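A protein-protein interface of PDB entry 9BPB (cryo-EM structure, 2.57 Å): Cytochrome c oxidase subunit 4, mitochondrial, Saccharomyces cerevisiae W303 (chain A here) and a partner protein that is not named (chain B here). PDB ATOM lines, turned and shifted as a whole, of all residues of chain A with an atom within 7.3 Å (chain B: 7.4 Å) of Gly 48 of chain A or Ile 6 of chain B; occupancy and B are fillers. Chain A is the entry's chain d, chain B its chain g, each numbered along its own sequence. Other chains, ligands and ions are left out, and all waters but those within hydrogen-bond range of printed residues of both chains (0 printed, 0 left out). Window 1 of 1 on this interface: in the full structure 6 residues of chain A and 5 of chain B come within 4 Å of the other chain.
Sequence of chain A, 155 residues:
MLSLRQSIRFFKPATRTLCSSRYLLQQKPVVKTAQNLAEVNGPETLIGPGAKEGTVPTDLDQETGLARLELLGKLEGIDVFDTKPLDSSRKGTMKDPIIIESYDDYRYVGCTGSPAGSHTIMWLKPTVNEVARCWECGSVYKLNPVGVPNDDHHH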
ATOM      1  N   THR A  33      -8.542  -2.866   4.051  1.00  0.00           N
ATOM      2  CA  THR A  33      -9.934  -3.161   3.743  1.00  0.00           C
ATOM      3  C   THR A  33     -10.319  -2.528   2.408  1.00  0.00           C
ATOM      4  O   THR A  33      -9.844  -1.449   2.047  1.00  0.00           O
ATOM      5  CB  THR A  33     -10.840  -2.650   4.866  1.00  0.00           C
ATOM      6  OG1 THR A  33     -10.439  -3.250   6.105  1.00  0.00           O
ATOM      7  CG2 THR A  33     -12.289  -3.017   4.603  1.00  0.00           C
ATOM      8  N   ALA A  34     -11.187  -3.224   1.669  1.00  0.00           N
ATOM      9  CA  ALA A  34     -11.436  -2.878   0.273  1.00  0.00           C
ATOM     10  C   ALA A  34     -12.004  -1.470   0.127  1.00  0.00           C
ATOM     11  O   ALA A  34     -11.574  -0.708  -0.746  1.00  0.00           O
ATOM     12  CB  ALA A  34     -12.378  -3.907  -0.353  1.00  0.00           C
ATOM     13  N   GLN A  35     -12.988  -1.116   0.956  1.00  0.00           N
ATOM     14  CA  GLN A  35     -13.704   0.161   0.936  1.00  0.00           C
ATOM     15  C   GLN A  35     -14.575   0.327  -0.305  1.00  0.00           C
ATOM     16  O   GLN A  35     -15.290   1.332  -0.409  1.00  0.00           O
ATOM     17  CB  GLN A  35     -12.768   1.375   1.036  1.00  0.00           C
ATOM     18  CG  GLN A  35     -11.970   1.472   2.328  1.00  0.00           C
ATOM     19  CD  GLN A  35     -12.854   1.569   3.557  1.00  0.00           C
ATOM     20  OE1 GLN A  35     -12.894   0.660   4.384  1.00  0.00           O
ATOM     21  NE2 GLN A  35     -13.571   2.681   3.681  1.00  0.00           N
ATOM     22  N   PRO A  43     -11.563 -12.455   0.347  1.00  0.00           N
ATOM     23  CA  PRO A  43     -11.845 -12.218   1.779  1.00  0.00           C
ATOM     24  C   PRO A  43     -10.985 -11.257   2.620  1.00  0.00           C
ATOM     25  O   PRO A  43     -11.561 -10.542   3.417  1.00  0.00           O
ATOM     26  CB  PRO A  43     -11.670 -13.621   2.391  1.00  0.00           C
ATOM     27  CG  PRO A  43     -10.703 -14.312   1.462  1.00  0.00           C
ATOM     28  CD  PRO A  43     -11.102 -13.820   0.088  1.00  0.00           C
ATOM     29  N   GLU A  44      -9.657 -11.248   2.442  1.00  0.00           N
ATOM     30  CA  GLU A  44      -8.796 -10.466   3.380  1.00  0.00           C
ATOM     31  C   GLU A  44      -9.140  -8.978   3.308  1.00  0.00           C
ATOM     32  O   GLU A  44      -9.207  -8.335   4.366  1.00  0.00           O
ATOM     33  CB  GLU A  44      -7.311 -10.725   3.115  1.00  0.00           C
ATOM     34  CG  GLU A  44      -6.561 -11.165   4.358  1.00  0.00           C
ATOM     35  CD  GLU A  44      -6.222 -10.049   5.333  1.00  0.00           C
ATOM     36  OE1 GLU A  44      -6.390  -8.872   4.964  1.00  0.00           O
ATOM     37  OE2 GLU A  44      -5.814 -10.360   6.467  1.00  0.00           O
ATOM     38  N   THR A  45      -9.379  -8.473   2.105  1.00  0.00           N
ATOM     39  CA  THR A  45      -9.757  -7.050   1.944  1.00  0.00           C
ATOM     40  C   THR A  45     -11.079  -6.791   2.662  1.00  0.00           C
ATOM     41  O   THR A  45     -11.215  -5.723   3.253  1.00  0.00           O
ATOM     42  CB  THR A  45      -9.889  -6.670   0.470  1.00  0.00           C
ATOM     43  OG1 THR A  45     -11.237  -6.953   0.104  1.00  0.00           O
ATOM     44  CG2 THR A  45      -8.894  -7.407  -0.399  1.00  0.00           C
ATOM     45  N   LEU A  46     -12.018  -7.729   2.624  1.00  0.00           N
ATOM     46  CA  LEU A  46     -13.327  -7.389   3.238  1.00  0.00           C
ATOM     47  C   LEU A  46     -13.141  -7.072   4.730  1.00  0.00           C
ATOM     48  O   LEU A  46     -13.680  -6.038   5.148  1.00  0.00           O
ATOM     49  CB  LEU A  46     -14.301  -8.548   3.004  1.00  0.00           C
ATOM     50  CG  LEU A  46     -14.775  -8.697   1.559  1.00  0.00           C
ATOM     51  CD1 LEU A  46     -15.850  -9.765   1.437  1.00  0.00           C
ATOM     52  CD2 LEU A  46     -15.285  -7.370   1.022  1.00  0.00           C
ATOM     53  N   ILE A  47     -12.337  -7.846   5.473  1.00  0.00           N
ATOM     54  CA  ILE A  47     -12.136  -7.618   6.945  1.00  0.00           C
ATOM     55  C   ILE A  47     -12.022  -6.111   7.192  1.00  0.00           C
ATOM     56  O   ILE A  47     -11.387  -5.428   6.354  1.00  0.00           O
ATOM     57  CB  ILE A  47     -10.922  -8.398   7.501  1.00  0.00           C
ATOM     58  CG1 ILE A  47      -9.609  -7.625   7.355  1.00  0.00           C
ATOM     59  CG2 ILE A  47     -10.833  -9.780   6.869  1.00  0.00           C
ATOM     60  CD1 ILE A  47      -8.399  -8.380   7.845  1.00  0.00           C
ATOM     61  N   GLY A  48     -12.524  -5.611   8.325  1.00  0.00           N
ATOM     62  CA  GLY A  48     -12.590  -4.187   8.541  1.00  0.00           C
ATOM     63  C   GLY A  48     -11.893  -3.746   9.809  1.00  0.00           C
ATOM     64  O   GLY A  48     -11.350  -4.557  10.564  1.00  0.00           O
ATOM     65  N   PRO A  49     -11.880  -2.439  10.060  1.00  0.00           N
ATOM     66  CA  PRO A  49     -11.315  -1.940  11.317  1.00  0.00           C
ATOM     67  C   PRO A  49     -12.312  -2.085  12.455  1.00  0.00           C
ATOM     68  O   PRO A  49     -13.494  -1.765  12.313  1.00  0.00           O
ATOM     69  CB  PRO A  49     -11.021  -0.469  11.011  1.00  0.00           C
ATOM     70  CG  PRO A  49     -12.034  -0.109   9.983  1.00  0.00           C
ATOM     71  CD  PRO A  49     -12.250  -1.343   9.148  1.00  0.00           C
ATOM     72  N   GLY A  50     -11.823  -2.565  13.594  1.00  0.00           N
ATOM     73  CA  GLY A  50     -12.697  -2.817  14.717  1.00  0.00           C
ATOM     74  C   GLY A  50     -13.220  -1.543  15.348  1.00  0.00           C
ATOM     75  O   GLY A  50     -12.705  -0.445  15.140  1.00  0.00           O
ATOM     76  N   ALA A  51     -14.278  -1.700  16.137  1.00  0.00           N
ATOM     77  CA  ALA A  51     -14.877  -0.564  16.819  1.00  0.00           C
ATOM     78  C   ALA A  51     -13.968  -0.067  17.936  1.00  0.00           C
ATOM     79  O   ALA A  51     -13.352  -0.856  18.657  1.00  0.00           O
ATOM     80  CB  ALA A  51     -16.241  -0.941  17.389  1.00  0.00           C
ATOM     81  N   ASP A  59     -21.778  -1.835  11.140  1.00  0.00           N
ATOM     82  CA  ASP A  59     -21.572  -2.912  10.175  1.00  0.00           C
ATOM     83  C   ASP A  59     -20.341  -2.657   9.316  1.00  0.00           C
ATOM     84  O   ASP A  59     -19.639  -3.599   8.935  1.00  0.00           O
ATOM     85  CB  ASP A  59     -22.814  -3.084   9.305  1.00  0.00           C
ATOM     86  CG  ASP A  59     -24.002  -3.599  10.086  1.00  0.00           C
ATOM     87  OD1 ASP A  59     -23.786  -4.252  11.128  1.00  0.00           O
ATOM     88  OD2 ASP A  59     -25.149  -3.357   9.658  1.00  0.00           O
ATOM     89  N   LEU A  60     -20.055  -1.391   9.011  1.00  0.00           N
ATOM     90  CA  LEU A  60     -18.843  -1.080   8.261  1.00  0.00           C
ATOM     91  C   LEU A  60     -17.588  -1.291   9.093  1.00  0.00           C
ATOM     92  O   LEU A  60     -16.480  -1.220   8.554  1.00  0.00           O
ATOM     93  CB  LEU A  60     -18.895   0.357   7.741  1.00  0.00           C
ATOM     94  CG  LEU A  60     -19.668   0.558   6.438  1.00  0.00           C
ATOM     95  CD1 LEU A  60     -19.803   2.035   6.109  1.00  0.00           C
ATOM     96  CD2 LEU A  60     -18.992  -0.185   5.299  1.00  0.00           C
ATOM     97  N   ASP A  61     -17.737  -1.543  10.395  1.00  0.00           N
ATOM     98  CA  ASP A  61     -16.581  -1.803  11.243  1.00  0.00           C
ATOM     99  C   ASP A  61     -16.306  -3.297  11.375  1.00  0.00           C
ATOM    100  O   ASP A  61     -15.160  -3.736  11.236  1.00  0.00           O
ATOM    101  CB  ASP A  61     -16.790  -1.180  12.622  1.00  0.00           C
ATOM    102  CG  ASP A  61     -16.718   0.331  12.596  1.00  0.00           C
ATOM    103  OD1 ASP A  61     -16.040   0.878  11.702  1.00  0.00           O
ATOM    104  OD2 ASP A  61     -17.337   0.972  13.470  1.00  0.00           O
ATOM    105  N   GLN A  62     -17.339  -4.095  11.638  1.00  0.00           N
ATOM    106  CA  GLN A  62     -17.148  -5.481  12.045  1.00  0.00           C
ATOM    107  C   GLN A  62     -17.926  -6.472  11.181  1.00  0.00           C
ATOM    108  O   GLN A  62     -18.563  -7.389  11.701  1.00  0.00           O
ATOM    109  CB  GLN A  62     -17.519  -5.654  13.517  1.00  0.00           C
ATOM    110  CG  GLN A  62     -16.331  -5.553  14.455  1.00  0.00           C
ATOM    111  CD  GLN A  62     -16.744  -5.362  15.898  1.00  0.00           C
ATOM    112  OE1 GLN A  62     -17.920  -5.482  16.240  1.00  0.00           O
ATOM    113  NE2 GLN A  62     -15.778  -5.058  16.753  1.00  0.00           N
ATOM    114  N   GLU A  63     -17.888  -6.302   9.863  1.00  0.00           N
ATOM    115  CA  GLU A  63     -18.290  -7.360   8.948  1.00  0.00           C
ATOM    116  C   GLU A  63     -17.038  -8.011   8.374  1.00  0.00           C
ATOM    117  O   GLU A  63     -15.989  -7.374   8.259  1.00  0.00           O
ATOM    118  CB  GLU A  63     -19.176  -6.818   7.826  1.00  0.00           C
ATOM    119  CG  GLU A  63     -20.600  -6.482   8.250  1.00  0.00           C
ATOM    120  CD  GLU A  63     -21.421  -7.705   8.607  1.00  0.00           C
ATOM    121  OE1 GLU A  63     -21.161  -8.788   8.045  1.00  0.00           O
ATOM    122  OE2 GLU A  63     -22.330  -7.583   9.454  1.00  0.00           O
ATOM    123  N   THR A  64     -17.142  -9.297   8.031  1.00  0.00           N
ATOM    124  CA  THR A  64     -15.944 -10.055   7.690  1.00  0.00           C
ATOM    125  C   THR A  64     -16.009 -10.875   6.408  1.00  0.00           C
ATOM    126  O   THR A  64     -14.953 -11.110   5.811  1.00  0.00           O
ATOM    127  CB  THR A  64     -15.561 -10.994   8.845  1.00  0.00           C
ATOM    128  OG1 THR A  64     -14.375 -11.718   8.499  1.00  0.00           O
ATOM    129  CG2 THR A  64     -16.683 -11.968   9.145  1.00  0.00           C
ATOM    130  N   ARG A  68     -20.336  -9.202   4.274  1.00  0.00           N
ATOM    131  CA  ARG A  68     -19.746  -7.893   4.008  1.00  0.00           C
ATOM    132  C   ARG A  68     -19.762  -7.567   2.521  1.00  0.00           C
ATOM    133  O   ARG A  68     -19.993  -6.415   2.137  1.00  0.00           O
ATOM    134  CB  ARG A  68     -18.318  -7.836   4.545  1.00  0.00           C
ATOM    135  CG  ARG A  68     -17.665  -6.482   4.353  1.00  0.00           C
ATOM    136  CD  ARG A  68     -16.526  -6.263   5.322  1.00  0.00           C
ATOM    137  NE  ARG A  68     -15.928  -4.943   5.161  1.00  0.00           N
ATOM    138  CZ  ARG A  68     -15.887  -4.022   6.114  1.00  0.00           C
ATOM    139  NH1 ARG A  68     -16.393  -4.246   7.314  1.00  0.00           N
ATOM    140  NH2 ARG A  68     -15.329  -2.844   5.854  1.00  0.00           N
ATOM    141  N   ASN B   3     -13.221  -5.070  19.547  1.00  0.00           N
ATOM    142  CA  ASN B   3     -12.274  -5.509  20.565  1.00  0.00           C
ATOM    143  C   ASN B   3     -11.335  -6.568  19.986  1.00  0.00           C
ATOM    144  O   ASN B   3     -10.594  -6.296  19.042  1.00  0.00           O
ATOM    145  CB  ASN B   3     -13.018  -6.051  21.789  1.00  0.00           C
ATOM    146  CG  ASN B   3     -12.131  -6.160  23.012  1.00  0.00           C
ATOM    147  OD1 ASN B   3     -11.039  -5.594  23.051  1.00  0.00           O
ATOM    148  ND2 ASN B   3     -12.597  -6.886  24.020  1.00  0.00           N
ATOM    149  N   LYS B   4     -11.375  -7.777  20.543  1.00  0.00           N
ATOM    150  CA  LYS B   4     -10.583  -8.889  20.037  1.00  0.00           C
ATOM    151  C   LYS B   4     -11.198  -9.540  18.807  1.00  0.00           C
ATOM    152  O   LYS B   4     -10.612 -10.486  18.269  1.00  0.00           O
ATOM    153  CB  LYS B   4     -10.395  -9.955  21.121  1.00  0.00           C
ATOM    154  CG  LYS B   4      -9.547  -9.527  22.298  1.00  0.00           C
ATOM    155  CD  LYS B   4      -9.249 -10.717  23.191  1.00  0.00           C
ATOM    156  CE  LYS B   4     -10.496 -11.184  23.919  1.00  0.00           C
ATOM    157  NZ  LYS B   4     -10.205 -12.284  24.879  1.00  0.00           N
ATOM    158  N   VAL B   5     -12.364  -9.067  18.363  1.00  0.00           N
ATOM    159  CA  VAL B   5     -13.068  -9.721  17.263  1.00  0.00           C
ATOM    160  C   VAL B   5     -12.223  -9.706  15.997  1.00  0.00           C
ATOM    161  O   VAL B   5     -12.203 -10.682  15.238  1.00  0.00           O
ATOM    162  CB  VAL B   5     -14.441  -9.056  17.043  1.00  0.00           C
ATOM    163  CG1 VAL B   5     -15.143  -9.665  15.848  1.00  0.00           C
ATOM    164  CG2 VAL B   5     -15.298  -9.192  18.290  1.00  0.00           C
ATOM    165  N   ILE B   6     -11.507  -8.608  15.752  1.00  0.00           N
ATOM    166  CA  ILE B   6     -10.691  -8.511  14.543  1.00  0.00           C
ATOM    167  C   ILE B   6      -9.561  -9.534  14.566  1.00  0.00           C
ATOM    168  O   ILE B   6      -9.302 -10.216  13.568  1.00  0.00           O
ATOM    169  CB  ILE B   6     -10.155  -7.079  14.373  1.00  0.00           C
ATOM    170  CG1 ILE B   6     -11.304  -6.130  14.038  1.00  0.00           C
ATOM    171  CG2 ILE B   6      -9.091  -7.033  13.295  1.00  0.00           C
ATOM    172  CD1 ILE B   6     -12.146  -6.598  12.875  1.00  0.00           C
ATOM    173  N   GLN B   7      -8.871  -9.663  15.702  1.00  0.00           N
ATOM    174  CA  GLN B   7      -7.787 -10.635  15.783  1.00  0.00           C
ATOM    175  C   GLN B   7      -8.305 -12.057  15.951  1.00  0.00           C
ATOM    176  O   GLN B   7      -7.573 -13.007  15.656  1.00  0.00           O
ATOM    177  CB  GLN B   7      -6.835 -10.285  16.928  1.00  0.00           C
ATOM    178  CG  GLN B   7      -7.382 -10.558  18.311  1.00  0.00           C
ATOM    179  CD  GLN B   7      -6.464 -10.058  19.405  1.00  0.00           C
ATOM    180  OE1 GLN B   7      -5.444  -9.427  19.132  1.00  0.00           O
ATOM    181  NE2 GLN B   7      -6.815 -10.346  20.651  1.00  0.00           N
ATOM    182  N   LEU B   8      -9.540 -12.227  16.428  1.00  0.00           N
ATOM    183  CA  LEU B   8     -10.166 -13.544  16.417  1.00  0.00           C
ATOM    184  C   LEU B   8     -10.667 -13.918  15.030  1.00  0.00           C
ATOM    185  O   LEU B   8     -10.710 -15.107  14.690  1.00  0.00           O
ATOM    186  CB  LEU B   8     -11.315 -13.593  17.421  1.00  0.00           C
ATOM    187  CG  LEU B   8     -11.012 -14.275  18.754  1.00  0.00           C
ATOM    188  CD1 LEU B   8     -12.274 -14.424  19.580  1.00  0.00           C
ATOM    189  CD2 LEU B   8     -10.362 -15.627  18.519  1.00  0.00           C
ATOM    190  N   GLN B   9     -11.056 -12.928  14.223  1.00  0.00           N
ATOM    191  CA  GLN B   9     -11.476 -13.208  12.854  1.00  0.00           C
ATOM    192  C   GLN B   9     -10.320 -13.753  12.027  1.00  0.00           C
ATOM    193  O   GLN B   9     -10.498 -14.688  11.240  1.00  0.00           O
ATOM    194  CB  GLN B   9     -12.051 -11.946  12.211  1.00  0.00           C
ATOM    195  CG  GLN B   9     -13.503 -11.674  12.571  1.00  0.00           C
ATOM    196  CD  GLN B   9     -14.021 -10.371  12.000  1.00  0.00           C
ATOM    197  OE1 GLN B   9     -13.342  -9.704  11.223  1.00  0.00           O
ATOM    198  NE2 GLN B   9     -15.238 -10.000  12.385  1.00  0.00           N
ATOM    199  N   LYS B  10      -9.125 -13.183  12.195  1.00  0.00           N
ATOM    200  CA  LYS B  10      -7.975 -13.625  11.414  1.00  0.00           C
ATOM    201  C   LYS B  10      -7.526 -15.026  11.807  1.00  0.00           C
ATOM    202  O   LYS B  10      -6.868 -15.707  11.014  1.00  0.00           O
ATOM    203  CB  LYS B  10      -6.820 -12.640  11.579  1.00  0.00           C
ATOM    204  CG  LYS B  10      -7.131 -11.230  11.116  1.00  0.00           C
ATOM    205  CD  LYS B  10      -6.040 -10.263  11.536  1.00  0.00           C
ATOM    206  CE  LYS B  10      -6.303  -8.865  11.009  1.00  0.00           C
ATOM    207  NZ  LYS B  10      -5.399  -7.854  11.621  1.00  0.00           N
ATOM    208  N   ILE B  11      -7.862 -15.470  13.018  1.00  0.00           N
ATOM    209  CA  ILE B  11      -7.435 -16.790  13.472  1.00  0.00           C
ATOM    210  C   ILE B  11      -8.399 -17.864  12.984  1.00  0.00           C
ATOM    211  O   ILE B  11      -7.978 -18.907  12.467  1.00  0.00           O
ATOM    212  CB  ILE B  11      -7.292 -16.809  15.004  1.00  0.00           C
ATOM    213  CG1 ILE B  11      -6.164 -15.877  15.440  1.00  0.00           C
ATOM    214  CG2 ILE B  11      -7.044 -18.220  15.502  1.00  0.00           C
ATOM    215  CD1 ILE B  11      -5.996 -15.784  16.935  1.00  0.00           C
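Gly 48 of chain A touches just one residue of chain B: Ile 6 (3.2 Å).
Printed residues of chain B within 4 Å of Gly 50 of chain A: Ile 6 (3.6 Å).
Of the printed residues of chain B, Thr 64 of chain A touches Gln 9.
Printed residues of chain A within 4 Å of Asn 3 of chain B: Gln 62 (3.8 Å).
Ile 6 of chain B touches two residues of chain A.
Of the printed residues of chain A, Gln 9 of chain B touches Thr 64 (3.5 Å).
Of the printed residues of chain A, Lys 10 of chain B touches Ile 47 (3.8 Å).
The nearest residue of chain B that does not touch Gly 48 of chain A is Gln 9 of chain B (5.1 Å).
The nearest printed residue of chain A that does not touch Ile 6 of chain B is Pro 49 of chain A (4.5 Å).
Among the printed residues, merely in contact across the chains: Gly 48 of chain A with Ile 6 of chain B, Thr 64 of chain A with Gln 9 of chain B, Gly 50 of chain A with Ile 6 of chain B, Gln 62 of chain A with Asn 3 of chain B and Ile 47 of chain A with Lys 10 of chain B.
Of the 9 printed residues of chain B, 4 touch a printed residue of chain A.
Along chain A the printed residues that touch a printed residue of chain B span positions 47 to 64.
Among the printed residues, no Asp or Glu carboxylate lies within 4 Å of a Lys or Arg side-chain nitrogen of the other chain.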
